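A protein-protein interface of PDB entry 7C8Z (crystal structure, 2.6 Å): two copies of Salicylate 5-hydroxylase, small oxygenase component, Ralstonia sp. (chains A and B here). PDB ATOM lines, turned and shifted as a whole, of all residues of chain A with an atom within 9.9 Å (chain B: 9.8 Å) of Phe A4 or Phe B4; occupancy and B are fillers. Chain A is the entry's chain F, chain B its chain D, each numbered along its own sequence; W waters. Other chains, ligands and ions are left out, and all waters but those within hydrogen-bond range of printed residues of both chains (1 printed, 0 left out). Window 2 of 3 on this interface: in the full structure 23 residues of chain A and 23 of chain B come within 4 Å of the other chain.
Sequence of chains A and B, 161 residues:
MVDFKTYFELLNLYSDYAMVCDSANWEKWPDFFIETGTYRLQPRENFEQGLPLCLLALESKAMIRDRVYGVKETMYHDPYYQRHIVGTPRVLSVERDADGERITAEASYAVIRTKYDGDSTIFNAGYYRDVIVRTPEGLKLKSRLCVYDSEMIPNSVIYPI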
ATOM      1  N   MET A   1       1.303 -11.992 -16.682  1.00  0.00           N
ATOM      2  CA  MET A   1       0.948 -10.602 -16.425  1.00  0.00           C
ATOM      3  C   MET A   1       1.642 -10.073 -15.169  1.00  0.00           C
ATOM      4  O   MET A   1       2.205  -8.974 -15.172  1.00  0.00           O
ATOM      5  CB  MET A   1      -0.568 -10.480 -16.278  1.00  0.00           C
ATOM      6  CG  MET A   1      -1.138  -9.165 -16.751  1.00  0.00           C
ATOM      7  SD  MET A   1      -2.895  -9.018 -16.380  1.00  0.00           S
ATOM      8  CE  MET A   1      -3.542  -8.683 -18.014  1.00  0.00           C
ATOM      9  N   VAL A   2       1.601 -10.867 -14.098  1.00  0.00           N
ATOM     10  CA  VAL A   2       2.378 -10.626 -12.888  1.00  0.00           C
ATOM     11  C   VAL A   2       2.969 -11.958 -12.447  1.00  0.00           C
ATOM     12  O   VAL A   2       2.363 -13.018 -12.628  1.00  0.00           O
ATOM     13  CB  VAL A   2       1.539  -9.994 -11.745  1.00  0.00           C
ATOM     14  CG1 VAL A   2       0.935  -8.668 -12.181  1.00  0.00           C
ATOM     15  CG2 VAL A   2       0.450 -10.942 -11.270  1.00  0.00           C
ATOM     16  N   ASP A   3       4.161 -11.904 -11.864  1.00  0.00           N
ATOM     17  CA  ASP A   3       4.759 -13.121 -11.339  1.00  0.00           C
ATOM     18  C   ASP A   3       4.244 -13.375  -9.920  1.00  0.00           C
ATOM     19  O   ASP A   3       3.516 -12.565  -9.342  1.00  0.00           O
ATOM     20  CB  ASP A   3       6.289 -13.046 -11.386  1.00  0.00           C
ATOM     21  CG  ASP A   3       6.863 -11.949 -10.513  1.00  0.00           C
ATOM     22  OD1 ASP A   3       6.099 -11.210  -9.866  1.00  0.00           O
ATOM     23  OD2 ASP A   3       8.105 -11.832 -10.474  1.00  0.00           O
ATOM     24  N   PHE A   4       4.616 -14.529  -9.360  1.00  0.00           N
ATOM     25  CA  PHE A   4       4.036 -14.917  -8.080  1.00  0.00           C
ATOM     26  C   PHE A   4       4.366 -13.912  -6.983  1.00  0.00           C
ATOM     27  O   PHE A   4       3.501 -13.577  -6.167  1.00  0.00           O
ATOM     28  CB  PHE A   4       4.498 -16.312  -7.668  1.00  0.00           C
ATOM     29  CG  PHE A   4       4.231 -16.613  -6.221  1.00  0.00           C
ATOM     30  CD1 PHE A   4       2.934 -16.683  -5.746  1.00  0.00           C
ATOM     31  CD2 PHE A   4       5.270 -16.777  -5.328  1.00  0.00           C
ATOM     32  CE1 PHE A   4       2.681 -16.937  -4.417  1.00  0.00           C
ATOM     33  CE2 PHE A   4       5.018 -17.030  -3.992  1.00  0.00           C
ATOM     34  CZ  PHE A   4       3.721 -17.107  -3.539  1.00  0.00           C
ATOM     35  N   LYS A   5       5.603 -13.407  -6.949  1.00  0.00           N
ATOM     36  CA  LYS A   5       5.971 -12.453  -5.905  1.00  0.00           C
ATOM     37  C   LYS A   5       5.101 -11.204  -5.967  1.00  0.00           C
ATOM     38  O   LYS A   5       4.614 -10.715  -4.939  1.00  0.00           O
ATOM     39  CB  LYS A   5       7.447 -12.081  -6.022  1.00  0.00           C
ATOM     40  CG  LYS A   5       8.053 -11.639  -4.705  1.00  0.00           C
ATOM     41  CD  LYS A   5       8.968 -10.439  -4.871  1.00  0.00           C
ATOM     42  CE  LYS A   5       9.455  -9.934  -3.514  1.00  0.00           C
ATOM     43  NZ  LYS A   5      10.245  -8.673  -3.621  1.00  0.00           N
ATOM     44  N   THR A   6       4.870 -10.687  -7.171  1.00  0.00           N
ATOM     45  CA  THR A   6       4.039  -9.494  -7.294  1.00  0.00           C
ATOM     46  C   THR A   6       2.590  -9.783  -6.923  1.00  0.00           C
ATOM     47  O   THR A   6       1.940  -8.966  -6.260  1.00  0.00           O
ATOM     48  CB  THR A   6       4.125  -8.937  -8.709  1.00  0.00           C
ATOM     49  OG1 THR A   6       5.502  -8.718  -9.041  1.00  0.00           O
ATOM     50  CG2 THR A   6       3.356  -7.624  -8.811  1.00  0.00           C
ATOM     51  N   TYR A   7       2.076 -10.945  -7.319  1.00  0.00           N
ATOM     52  CA  TYR A   7       0.699 -11.297  -6.983  1.00  0.00           C
ATOM     53  C   TYR A   7       0.522 -11.433  -5.477  1.00  0.00           C
ATOM     54  O   TYR A   7      -0.475 -10.967  -4.905  1.00  0.00           O
ATOM     55  CB  TYR A   7       0.324 -12.595  -7.691  1.00  0.00           C
ATOM     56  CG  TYR A   7      -1.142 -12.917  -7.678  1.00  0.00           C
ATOM     57  CD1 TYR A   7      -2.069 -12.052  -8.247  1.00  0.00           C
ATOM     58  CD2 TYR A   7      -1.604 -14.095  -7.106  1.00  0.00           C
ATOM     59  CE1 TYR A   7      -3.416 -12.352  -8.240  1.00  0.00           C
ATOM     60  CE2 TYR A   7      -2.949 -14.403  -7.093  1.00  0.00           C
ATOM     61  CZ  TYR A   7      -3.850 -13.529  -7.662  1.00  0.00           C
ATOM     62  OH  TYR A   7      -5.190 -13.838  -7.650  1.00  0.00           O
ATOM     63  N   PHE A   8       1.481 -12.089  -4.825  1.00  0.00           N
ATOM     64  CA  PHE A   8       1.492 -12.180  -3.373  1.00  0.00           C
ATOM     65  C   PHE A   8       1.469 -10.793  -2.741  1.00  0.00           C
ATOM     66  O   PHE A   8       0.634 -10.506  -1.874  1.00  0.00           O
ATOM     67  CB  PHE A   8       2.727 -12.968  -2.931  1.00  0.00           C
ATOM     68  CG  PHE A   8       2.919 -13.019  -1.445  1.00  0.00           C
ATOM     69  CD1 PHE A   8       2.208 -13.923  -0.675  1.00  0.00           C
ATOM     70  CD2 PHE A   8       3.818 -12.175  -0.819  1.00  0.00           C
ATOM     71  CE1 PHE A   8       2.379 -13.981   0.690  1.00  0.00           C
ATOM     72  CE2 PHE A   8       3.996 -12.231   0.547  1.00  0.00           C
ATOM     73  CZ  PHE A   8       3.272 -13.137   1.303  1.00  0.00           C
ATOM     74  N   GLU A   9       2.372  -9.912  -3.180  1.00  0.00           N
ATOM     75  CA  GLU A   9       2.419  -8.565  -2.617  1.00  0.00           C
ATOM     76  C   GLU A   9       1.130  -7.800  -2.887  1.00  0.00           C
ATOM     77  O   GLU A   9       0.714  -6.978  -2.068  1.00  0.00           O
ATOM     78  CB  GLU A   9       3.625  -7.804  -3.170  1.00  0.00           C
ATOM     79  CG  GLU A   9       4.957  -8.412  -2.764  1.00  0.00           C
ATOM     80  CD  GLU A   9       6.118  -7.457  -2.941  1.00  0.00           C
ATOM     81  OE1 GLU A   9       6.594  -7.308  -4.082  1.00  0.00           O
ATOM     82  OE2 GLU A   9       6.560  -6.860  -1.940  1.00  0.00           O
ATOM     83  N   LEU A  10       0.472  -8.072  -4.010  1.00  0.00           N
ATOM     84  CA  LEU A  10      -0.755  -7.360  -4.342  1.00  0.00           C
ATOM     85  C   LEU A  10      -1.907  -7.786  -3.437  1.00  0.00           C
ATOM     86  O   LEU A  10      -2.644  -6.939  -2.902  1.00  0.00           O
ATOM     87  CB  LEU A  10      -1.101  -7.591  -5.808  1.00  0.00           C
ATOM     88  CG  LEU A  10      -2.363  -6.865  -6.227  1.00  0.00           C
ATOM     89  CD1 LEU A  10      -2.046  -5.940  -7.384  1.00  0.00           C
ATOM     90  CD2 LEU A  10      -3.436  -7.877  -6.590  1.00  0.00           C
ATOM     91  N   LEU A  11      -2.100  -9.100  -3.283  1.00  0.00           N
ATOM     92  CA  LEU A  11      -3.126  -9.579  -2.359  1.00  0.00           C
ATOM     93  C   LEU A  11      -2.835  -9.106  -0.943  1.00  0.00           C
ATOM     94  O   LEU A  11      -3.753  -8.739  -0.195  1.00  0.00           O
ATOM     95  CB  LEU A  11      -3.230 -11.102  -2.416  1.00  0.00           C
ATOM     96  CG  LEU A  11      -3.589 -11.674  -3.793  1.00  0.00           C
ATOM     97  CD1 LEU A  11      -4.024 -13.134  -3.701  1.00  0.00           C
ATOM     98  CD2 LEU A  11      -4.657 -10.834  -4.475  1.00  0.00           C
ATOM     99  N   ASN A  12      -1.555  -9.089  -0.563  1.00  0.00           N
ATOM    100  CA  ASN A  12      -1.178  -8.547   0.735  1.00  0.00           C
ATOM    101  C   ASN A  12      -1.517  -7.067   0.839  1.00  0.00           C
ATOM    102  O   ASN A  12      -1.910  -6.599   1.906  1.00  0.00           O
ATOM    103  CB  ASN A  12       0.312  -8.767   0.984  1.00  0.00           C
ATOM    104  CG  ASN A  12       0.589  -9.995   1.821  1.00  0.00           C
ATOM    105  OD1 ASN A  12      -0.315 -10.565   2.435  1.00  0.00           O
ATOM    106  ND2 ASN A  12       1.848 -10.416   1.848  1.00  0.00           N
ATOM    107  N   VAL A  91      -6.766  -8.813 -11.435  1.00  0.00           N
ATOM    108  CA  VAL A  91      -5.718  -8.048 -12.102  1.00  0.00           C
ATOM    109  C   VAL A  91      -6.156  -7.829 -13.542  1.00  0.00           C
ATOM    110  O   VAL A  91      -6.412  -8.797 -14.269  1.00  0.00           O
ATOM    111  CB  VAL A  91      -4.366  -8.776 -12.047  1.00  0.00           C
ATOM    112  CG1 VAL A  91      -3.304  -7.985 -12.794  1.00  0.00           C
ATOM    113  CG2 VAL A  91      -3.946  -9.027 -10.606  1.00  0.00           C
ATOM    114  N   ARG A 134       5.138   0.133  -7.760  1.00  0.00           N
ATOM    115  CA  ARG A 134       6.123  -0.457  -6.868  1.00  0.00           C
ATOM    116  C   ARG A 134       7.115   0.610  -6.422  1.00  0.00           C
ATOM    117  O   ARG A 134       7.710   1.297  -7.257  1.00  0.00           O
ATOM    118  CB  ARG A 134       6.844  -1.608  -7.566  1.00  0.00           C
ATOM    119  CG  ARG A 134       7.969  -2.216  -6.763  1.00  0.00           C
ATOM    120  CD  ARG A 134       8.580  -3.398  -7.496  1.00  0.00           C
ATOM    121  NE  ARG A 134       7.707  -4.565  -7.470  1.00  0.00           N
ATOM    122  CZ  ARG A 134       7.500  -5.311  -6.391  1.00  0.00           C
ATOM    123  NH1 ARG A 134       8.103  -5.007  -5.247  1.00  0.00           N
ATOM    124  NH2 ARG A 134       6.690  -6.361  -6.453  1.00  0.00           N
ATOM    125  N   LEU A 139       4.542  -2.416  -2.728  1.00  0.00           N
ATOM    126  CA  LEU A 139       3.463  -1.919  -3.570  1.00  0.00           C
ATOM    127  C   LEU A 139       2.709  -0.816  -2.846  1.00  0.00           C
ATOM    128  O   LEU A 139       2.446  -0.908  -1.646  1.00  0.00           O
ATOM    129  CB  LEU A 139       2.499  -3.048  -3.951  1.00  0.00           C
ATOM    130  CG  LEU A 139       3.065  -4.127  -4.873  1.00  0.00           C
ATOM    131  CD1 LEU A 139       1.980  -5.060  -5.348  1.00  0.00           C
ATOM    132  CD2 LEU A 139       3.754  -3.480  -6.045  1.00  0.00           C
ATOM    133  N   MET B   1      -1.096 -29.245  -7.631  1.00  0.00           N
ATOM    134  CA  MET B   1      -2.419 -29.528  -8.165  1.00  0.00           C
ATOM    135  C   MET B   1      -2.716 -28.607  -9.334  1.00  0.00           C
ATOM    136  O   MET B   1      -3.209 -29.041 -10.374  1.00  0.00           O
ATOM    137  CB  MET B   1      -3.479 -29.358  -7.076  1.00  0.00           C
ATOM    138  CG  MET B   1      -4.707 -30.234  -7.260  1.00  0.00           C
ATOM    139  SD  MET B   1      -6.001 -29.871  -6.052  1.00  0.00           S
ATOM    140  CE  MET B   1      -5.847 -31.299  -4.986  1.00  0.00           C
ATOM    141  N   VAL B   2      -2.411 -27.326  -9.149  1.00  0.00           N
ATOM    142  CA  VAL B   2      -2.429 -26.342 -10.222  1.00  0.00           C
ATOM    143  C   VAL B   2      -1.184 -25.480 -10.086  1.00  0.00           C
ATOM    144  O   VAL B   2      -0.701 -25.231  -8.979  1.00  0.00           O
ATOM    145  CB  VAL B   2      -3.710 -25.482 -10.202  1.00  0.00           C
ATOM    146  CG1 VAL B   2      -4.932 -26.340 -10.509  1.00  0.00           C
ATOM    147  CG2 VAL B   2      -3.864 -24.785  -8.855  1.00  0.00           C
ATOM    148  N   ASP B   3      -0.663 -25.014 -11.215  1.00  0.00           N
ATOM    149  CA  ASP B   3       0.483 -24.123 -11.157  1.00  0.00           C
ATOM    150  C   ASP B   3       0.018 -22.684 -10.936  1.00  0.00           C
ATOM    151  O   ASP B   3      -1.178 -22.385 -10.922  1.00  0.00           O
ATOM    152  CB  ASP B   3       1.326 -24.241 -12.429  1.00  0.00           C
ATOM    153  CG  ASP B   3       0.544 -23.918 -13.693  1.00  0.00           C
ATOM    154  OD1 ASP B   3      -0.677 -23.665 -13.609  1.00  0.00           O
ATOM    155  OD2 ASP B   3       1.157 -23.925 -14.783  1.00  0.00           O
ATOM    156  N   PHE B   4       0.988 -21.785 -10.743  1.00  0.00           N
ATOM    157  CA  PHE B   4       0.651 -20.403 -10.408  1.00  0.00           C
ATOM    158  C   PHE B   4      -0.162 -19.745 -11.511  1.00  0.00           C
ATOM    159  O   PHE B   4      -1.090 -18.987 -11.227  1.00  0.00           O
ATOM    160  CB  PHE B   4       1.909 -19.582 -10.137  1.00  0.00           C
ATOM    161  CG  PHE B   4       1.658 -18.099 -10.089  1.00  0.00           C
ATOM    162  CD1 PHE B   4       0.828 -17.555  -9.121  1.00  0.00           C
ATOM    163  CD2 PHE B   4       2.246 -17.249 -11.012  1.00  0.00           C
ATOM    164  CE1 PHE B   4       0.588 -16.189  -9.069  1.00  0.00           C
ATOM    165  CE2 PHE B   4       2.010 -15.882 -10.970  1.00  0.00           C
ATOM    166  CZ  PHE B   4       1.176 -15.353  -9.995  1.00  0.00           C
ATOM    167  N   LYS B   5       0.178 -20.008 -12.775  1.00  0.00           N
ATOM    168  CA  LYS B   5      -0.566 -19.399 -13.874  1.00  0.00           C
ATOM    169  C   LYS B   5      -2.037 -19.793 -13.824  1.00  0.00           C
ATOM    170  O   LYS B   5      -2.930 -18.942 -13.933  1.00  0.00           O
ATOM    171  CB  LYS B   5       0.056 -19.814 -15.208  1.00  0.00           C
ATOM    172  CG  LYS B   5      -0.340 -18.946 -16.386  1.00  0.00           C
ATOM    173  CD  LYS B   5      -0.582 -19.779 -17.645  1.00  0.00           C
ATOM    174  CE  LYS B   5      -1.137 -18.923 -18.777  1.00  0.00           C
ATOM    175  NZ  LYS B   5      -1.597 -19.744 -19.933  1.00  0.00           N
ATOM    176  N   THR B   6      -2.307 -21.080 -13.600  1.00  0.00           N
ATOM    177  CA  THR B   6      -3.689 -21.538 -13.530  1.00  0.00           C
ATOM    178  C   THR B   6      -4.389 -21.004 -12.291  1.00  0.00           C
ATOM    179  O   THR B   6      -5.574 -20.665 -12.342  1.00  0.00           O
ATOM    180  CB  THR B   6      -3.738 -23.062 -13.550  1.00  0.00           C
ATOM    181  OG1 THR B   6      -2.956 -23.541 -14.647  1.00  0.00           O
ATOM    182  CG2 THR B   6      -5.167 -23.543 -13.698  1.00  0.00           C
ATOM    183  N   TYR B   7      -3.680 -20.933 -11.163  1.00  0.00           N
ATOM    184  CA  TYR B   7      -4.288 -20.404  -9.947  1.00  0.00           C
ATOM    185  C   TYR B   7      -4.655 -18.937 -10.119  1.00  0.00           C
ATOM    186  O   TYR B   7      -5.739 -18.502  -9.710  1.00  0.00           O
ATOM    187  CB  TYR B   7      -3.326 -20.585  -8.776  1.00  0.00           C
ATOM    188  CG  TYR B   7      -3.951 -20.357  -7.430  1.00  0.00           C
ATOM    189  CD1 TYR B   7      -4.932 -21.212  -6.947  1.00  0.00           C
ATOM    190  CD2 TYR B   7      -3.566 -19.288  -6.640  1.00  0.00           C
ATOM    191  CE1 TYR B   7      -5.506 -21.011  -5.715  1.00  0.00           C
ATOM    192  CE2 TYR B   7      -4.138 -19.076  -5.404  1.00  0.00           C
ATOM    193  CZ  TYR B   7      -5.109 -19.944  -4.945  1.00  0.00           C
ATOM    194  OH  TYR B   7      -5.684 -19.742  -3.711  1.00  0.00           O
ATOM    195  N   PHE B   8      -3.744 -18.165 -10.707  1.00  0.00           N
ATOM    196  CA  PHE B   8      -3.998 -16.772 -11.045  1.00  0.00           C
ATOM    197  C   PHE B   8      -5.236 -16.653 -11.918  1.00  0.00           C
ATOM    198  O   PHE B   8      -6.137 -15.855 -11.637  1.00  0.00           O
ATOM    199  CB  PHE B   8      -2.760 -16.203 -11.750  1.00  0.00           C
ATOM    200  CG  PHE B   8      -2.932 -14.814 -12.303  1.00  0.00           C
ATOM    201  CD1 PHE B   8      -2.629 -13.708 -11.531  1.00  0.00           C
ATOM    202  CD2 PHE B   8      -3.353 -14.618 -13.613  1.00  0.00           C
ATOM    203  CE1 PHE B   8      -2.768 -12.430 -12.039  1.00  0.00           C
ATOM    204  CE2 PHE B   8      -3.495 -13.342 -14.127  1.00  0.00           C
ATOM    205  CZ  PHE B   8      -3.204 -12.246 -13.337  1.00  0.00           C
ATOM    206  N   GLU B   9      -5.299 -17.454 -12.986  1.00  0.00           N
ATOM    207  CA  GLU B   9      -6.455 -17.401 -13.871  1.00  0.00           C
ATOM    208  C   GLU B   9      -7.734 -17.815 -13.160  1.00  0.00           C
ATOM    209  O   GLU B   9      -8.798 -17.269 -13.442  1.00  0.00           O
ATOM    210  CB  GLU B   9      -6.212 -18.282 -15.093  1.00  0.00           C
ATOM    211  CG  GLU B   9      -5.161 -17.739 -16.042  1.00  0.00           C
ATOM    212  CD  GLU B   9      -5.080 -18.544 -17.320  1.00  0.00           C
ATOM    213  OE1 GLU B   9      -4.277 -19.501 -17.370  1.00  0.00           O
ATOM    214  OE2 GLU B   9      -5.831 -18.232 -18.269  1.00  0.00           O
ATOM    215  N   LEU B  10      -7.646 -18.741 -12.209  1.00  0.00           N
ATOM    216  CA  LEU B  10      -8.837 -19.221 -11.512  1.00  0.00           C
ATOM    217  C   LEU B  10      -9.391 -18.159 -10.570  1.00  0.00           C
ATOM    218  O   LEU B  10     -10.603 -17.882 -10.559  1.00  0.00           O
ATOM    219  CB  LEU B  10      -8.490 -20.493 -10.746  1.00  0.00           C
ATOM    220  CG  LEU B  10      -9.628 -21.383 -10.272  1.00  0.00           C
ATOM    221  CD1 LEU B  10      -9.342 -22.794 -10.729  1.00  0.00           C
ATOM    222  CD2 LEU B  10      -9.749 -21.315  -8.760  1.00  0.00           C
ATOM    223  N   LEU B  11      -8.519 -17.570  -9.750  1.00  0.00           N
ATOM    224  CA  LEU B  11      -8.963 -16.483  -8.888  1.00  0.00           C
ATOM    225  C   LEU B  11      -9.496 -15.329  -9.720  1.00  0.00           C
ATOM    226  O   LEU B  11     -10.530 -14.738  -9.386  1.00  0.00           O
ATOM    227  CB  LEU B  11      -7.820 -16.018  -7.987  1.00  0.00           C
ATOM    228  CG  LEU B  11      -7.256 -17.070  -7.028  1.00  0.00           C
ATOM    229  CD1 LEU B  11      -6.488 -16.385  -5.908  1.00  0.00           C
ATOM    230  CD2 LEU B  11      -8.367 -17.965  -6.475  1.00  0.00           C
ATOM    231  N   ASN B  12      -8.827 -15.030 -10.840  1.00  0.00           N
ATOM    232  CA  ASN B  12      -9.321 -14.007 -11.750  1.00  0.00           C
ATOM    233  C   ASN B  12     -10.679 -14.378 -12.324  1.00  0.00           C
ATOM    234  O   ASN B  12     -11.502 -13.498 -12.554  1.00  0.00           O
ATOM    235  CB  ASN B  12      -8.312 -13.766 -12.869  1.00  0.00           C
ATOM    236  CG  ASN B  12      -7.405 -12.584 -12.590  1.00  0.00           C
ATOM    237  OD1 ASN B  12      -7.600 -11.853 -11.623  1.00  0.00           O
ATOM    238  ND2 ASN B  12      -6.419 -12.382 -13.447  1.00  0.00           N
ATOM    239  N   ARG B 134     -10.319 -25.295 -19.422  1.00  0.00           N
ATOM    240  CA  ARG B 134      -9.505 -24.328 -20.144  1.00  0.00           C
ATOM    241  C   ARG B 134      -9.883 -24.368 -21.617  1.00  0.00           C
ATOM    242  O   ARG B 134      -9.921 -25.445 -22.219  1.00  0.00           O
ATOM    243  CB  ARG B 134      -8.015 -24.617 -19.959  1.00  0.00           C
ATOM    244  CG  ARG B 134      -7.135 -23.930 -20.972  1.00  0.00           C
ATOM    245  CD  ARG B 134      -5.683 -23.922 -20.531  1.00  0.00           C
ATOM    246  NE  ARG B 134      -5.363 -22.740 -19.738  1.00  0.00           N
ATOM    247  CZ  ARG B 134      -5.139 -22.750 -18.428  1.00  0.00           C
ATOM    248  NH1 ARG B 134      -5.194 -23.890 -17.745  1.00  0.00           N
ATOM    249  NH2 ARG B 134      -4.853 -21.619 -17.799  1.00  0.00           N
ATOM    250  N   LEU B 139      -9.918 -19.706 -18.910  1.00  0.00           N
ATOM    251  CA  LEU B 139     -10.724 -20.604 -18.097  1.00  0.00           C
ATOM    252  C   LEU B 139     -12.202 -20.247 -18.232  1.00  0.00           C
ATOM    253  O   LEU B 139     -12.574 -19.071 -18.277  1.00  0.00           O
ATOM    254  CB  LEU B 139     -10.287 -20.548 -16.632  1.00  0.00           C
ATOM    255  CG  LEU B 139      -8.824 -20.881 -16.307  1.00  0.00           C
ATOM    256  CD1 LEU B 139      -8.620 -21.015 -14.814  1.00  0.00           C
ATOM    257  CD2 LEU B 139      -8.378 -22.149 -17.005  1.00  0.00           C
HETATM  258  O   HOH W   1      -6.488 -12.375  -9.103  1.00  0.00           O
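Water W1 bridges the side-chain hydroxyl (OH) of Tyr A7 and the side-chain amide oxygen (OD1) of Asn B12.
Phe B4 touches four residues of chain A. Of chain B, only Phe B4 comes within 4 Å of Asp A3. No residue of chain A comes within 4 Å of Asp B3. Of the printed residues of chain B, Val A91 touches Phe B8 (3.9 Å) and Asn B12 (3.2 Å). Printed residues of chain B within 4 Å of Val A2: Phe B4 and Phe B8. Of the printed residues of chain A, Asn B12 touches Val A91 (3.2 Å). Printed residues of chain A within 4 Å of Phe B8: Val A2 (3.6 Å), Tyr A7 (3.6 Å) and Val A91 (3.9 Å). Thr B6 touches none of the printed residues of chain A. Asn A12 touches none of the printed residues of chain B. The nearest residue of chain A that does not touch Phe B4 is Lys A5 (5.7 Å).
OG1 of Thr A6 is in hydrogen-bond range of OD1 of Asp A3, at 2.7 Å.
OD1 of Asn B12 is in hydrogen-bond range of N of Val A91 (3.2 Å).
Hydrophobic or aromatic side chains of chain B within 4 Å of the printed part of chain A: Phe B4, Phe B8 and Leu B11. Printed residues of chain A that touch a printed residue of chain B: Val A2, Asp A3, Phe A4, Tyr A7 and Val A91. Among the printed residues, 9 pairs touch across the chains.
Val A2 touches Phe B8, but with the chains exchanged Phe A8 does not touch Val B2 (14.0 Å). Phe A4 touches its own counterpart, Phe B4. Tyr A7 touches Phe B8, but with the chains exchanged Phe A8 does not touch Tyr B7 (9.0 Å). Tyr A7 touches Leu B11, but with the chains exchanged Leu A11 does not touch Tyr B7 (6.2 Å). Positions printed for both chains: 1, 2, 3, 4, 5, 6, 7, 8, 9, 10, 11, 12, 134 and 139.
Among the printed residues, pairs that only touch across the chains: Val A2 with Phe B4 (3.3 Å), Val A2 with Phe B8 (3.6 Å), Asp A3 with Phe B4 (3.5 Å), Phe A4 with Phe B4 (3.3 Å), Tyr A7 with Phe B4 (3.6 Å), Tyr A7 with Phe B8 (3.6 Å), Tyr A7 with Leu B11 (3.3 Å) and Val A91 with Phe B8 (3.9 Å).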
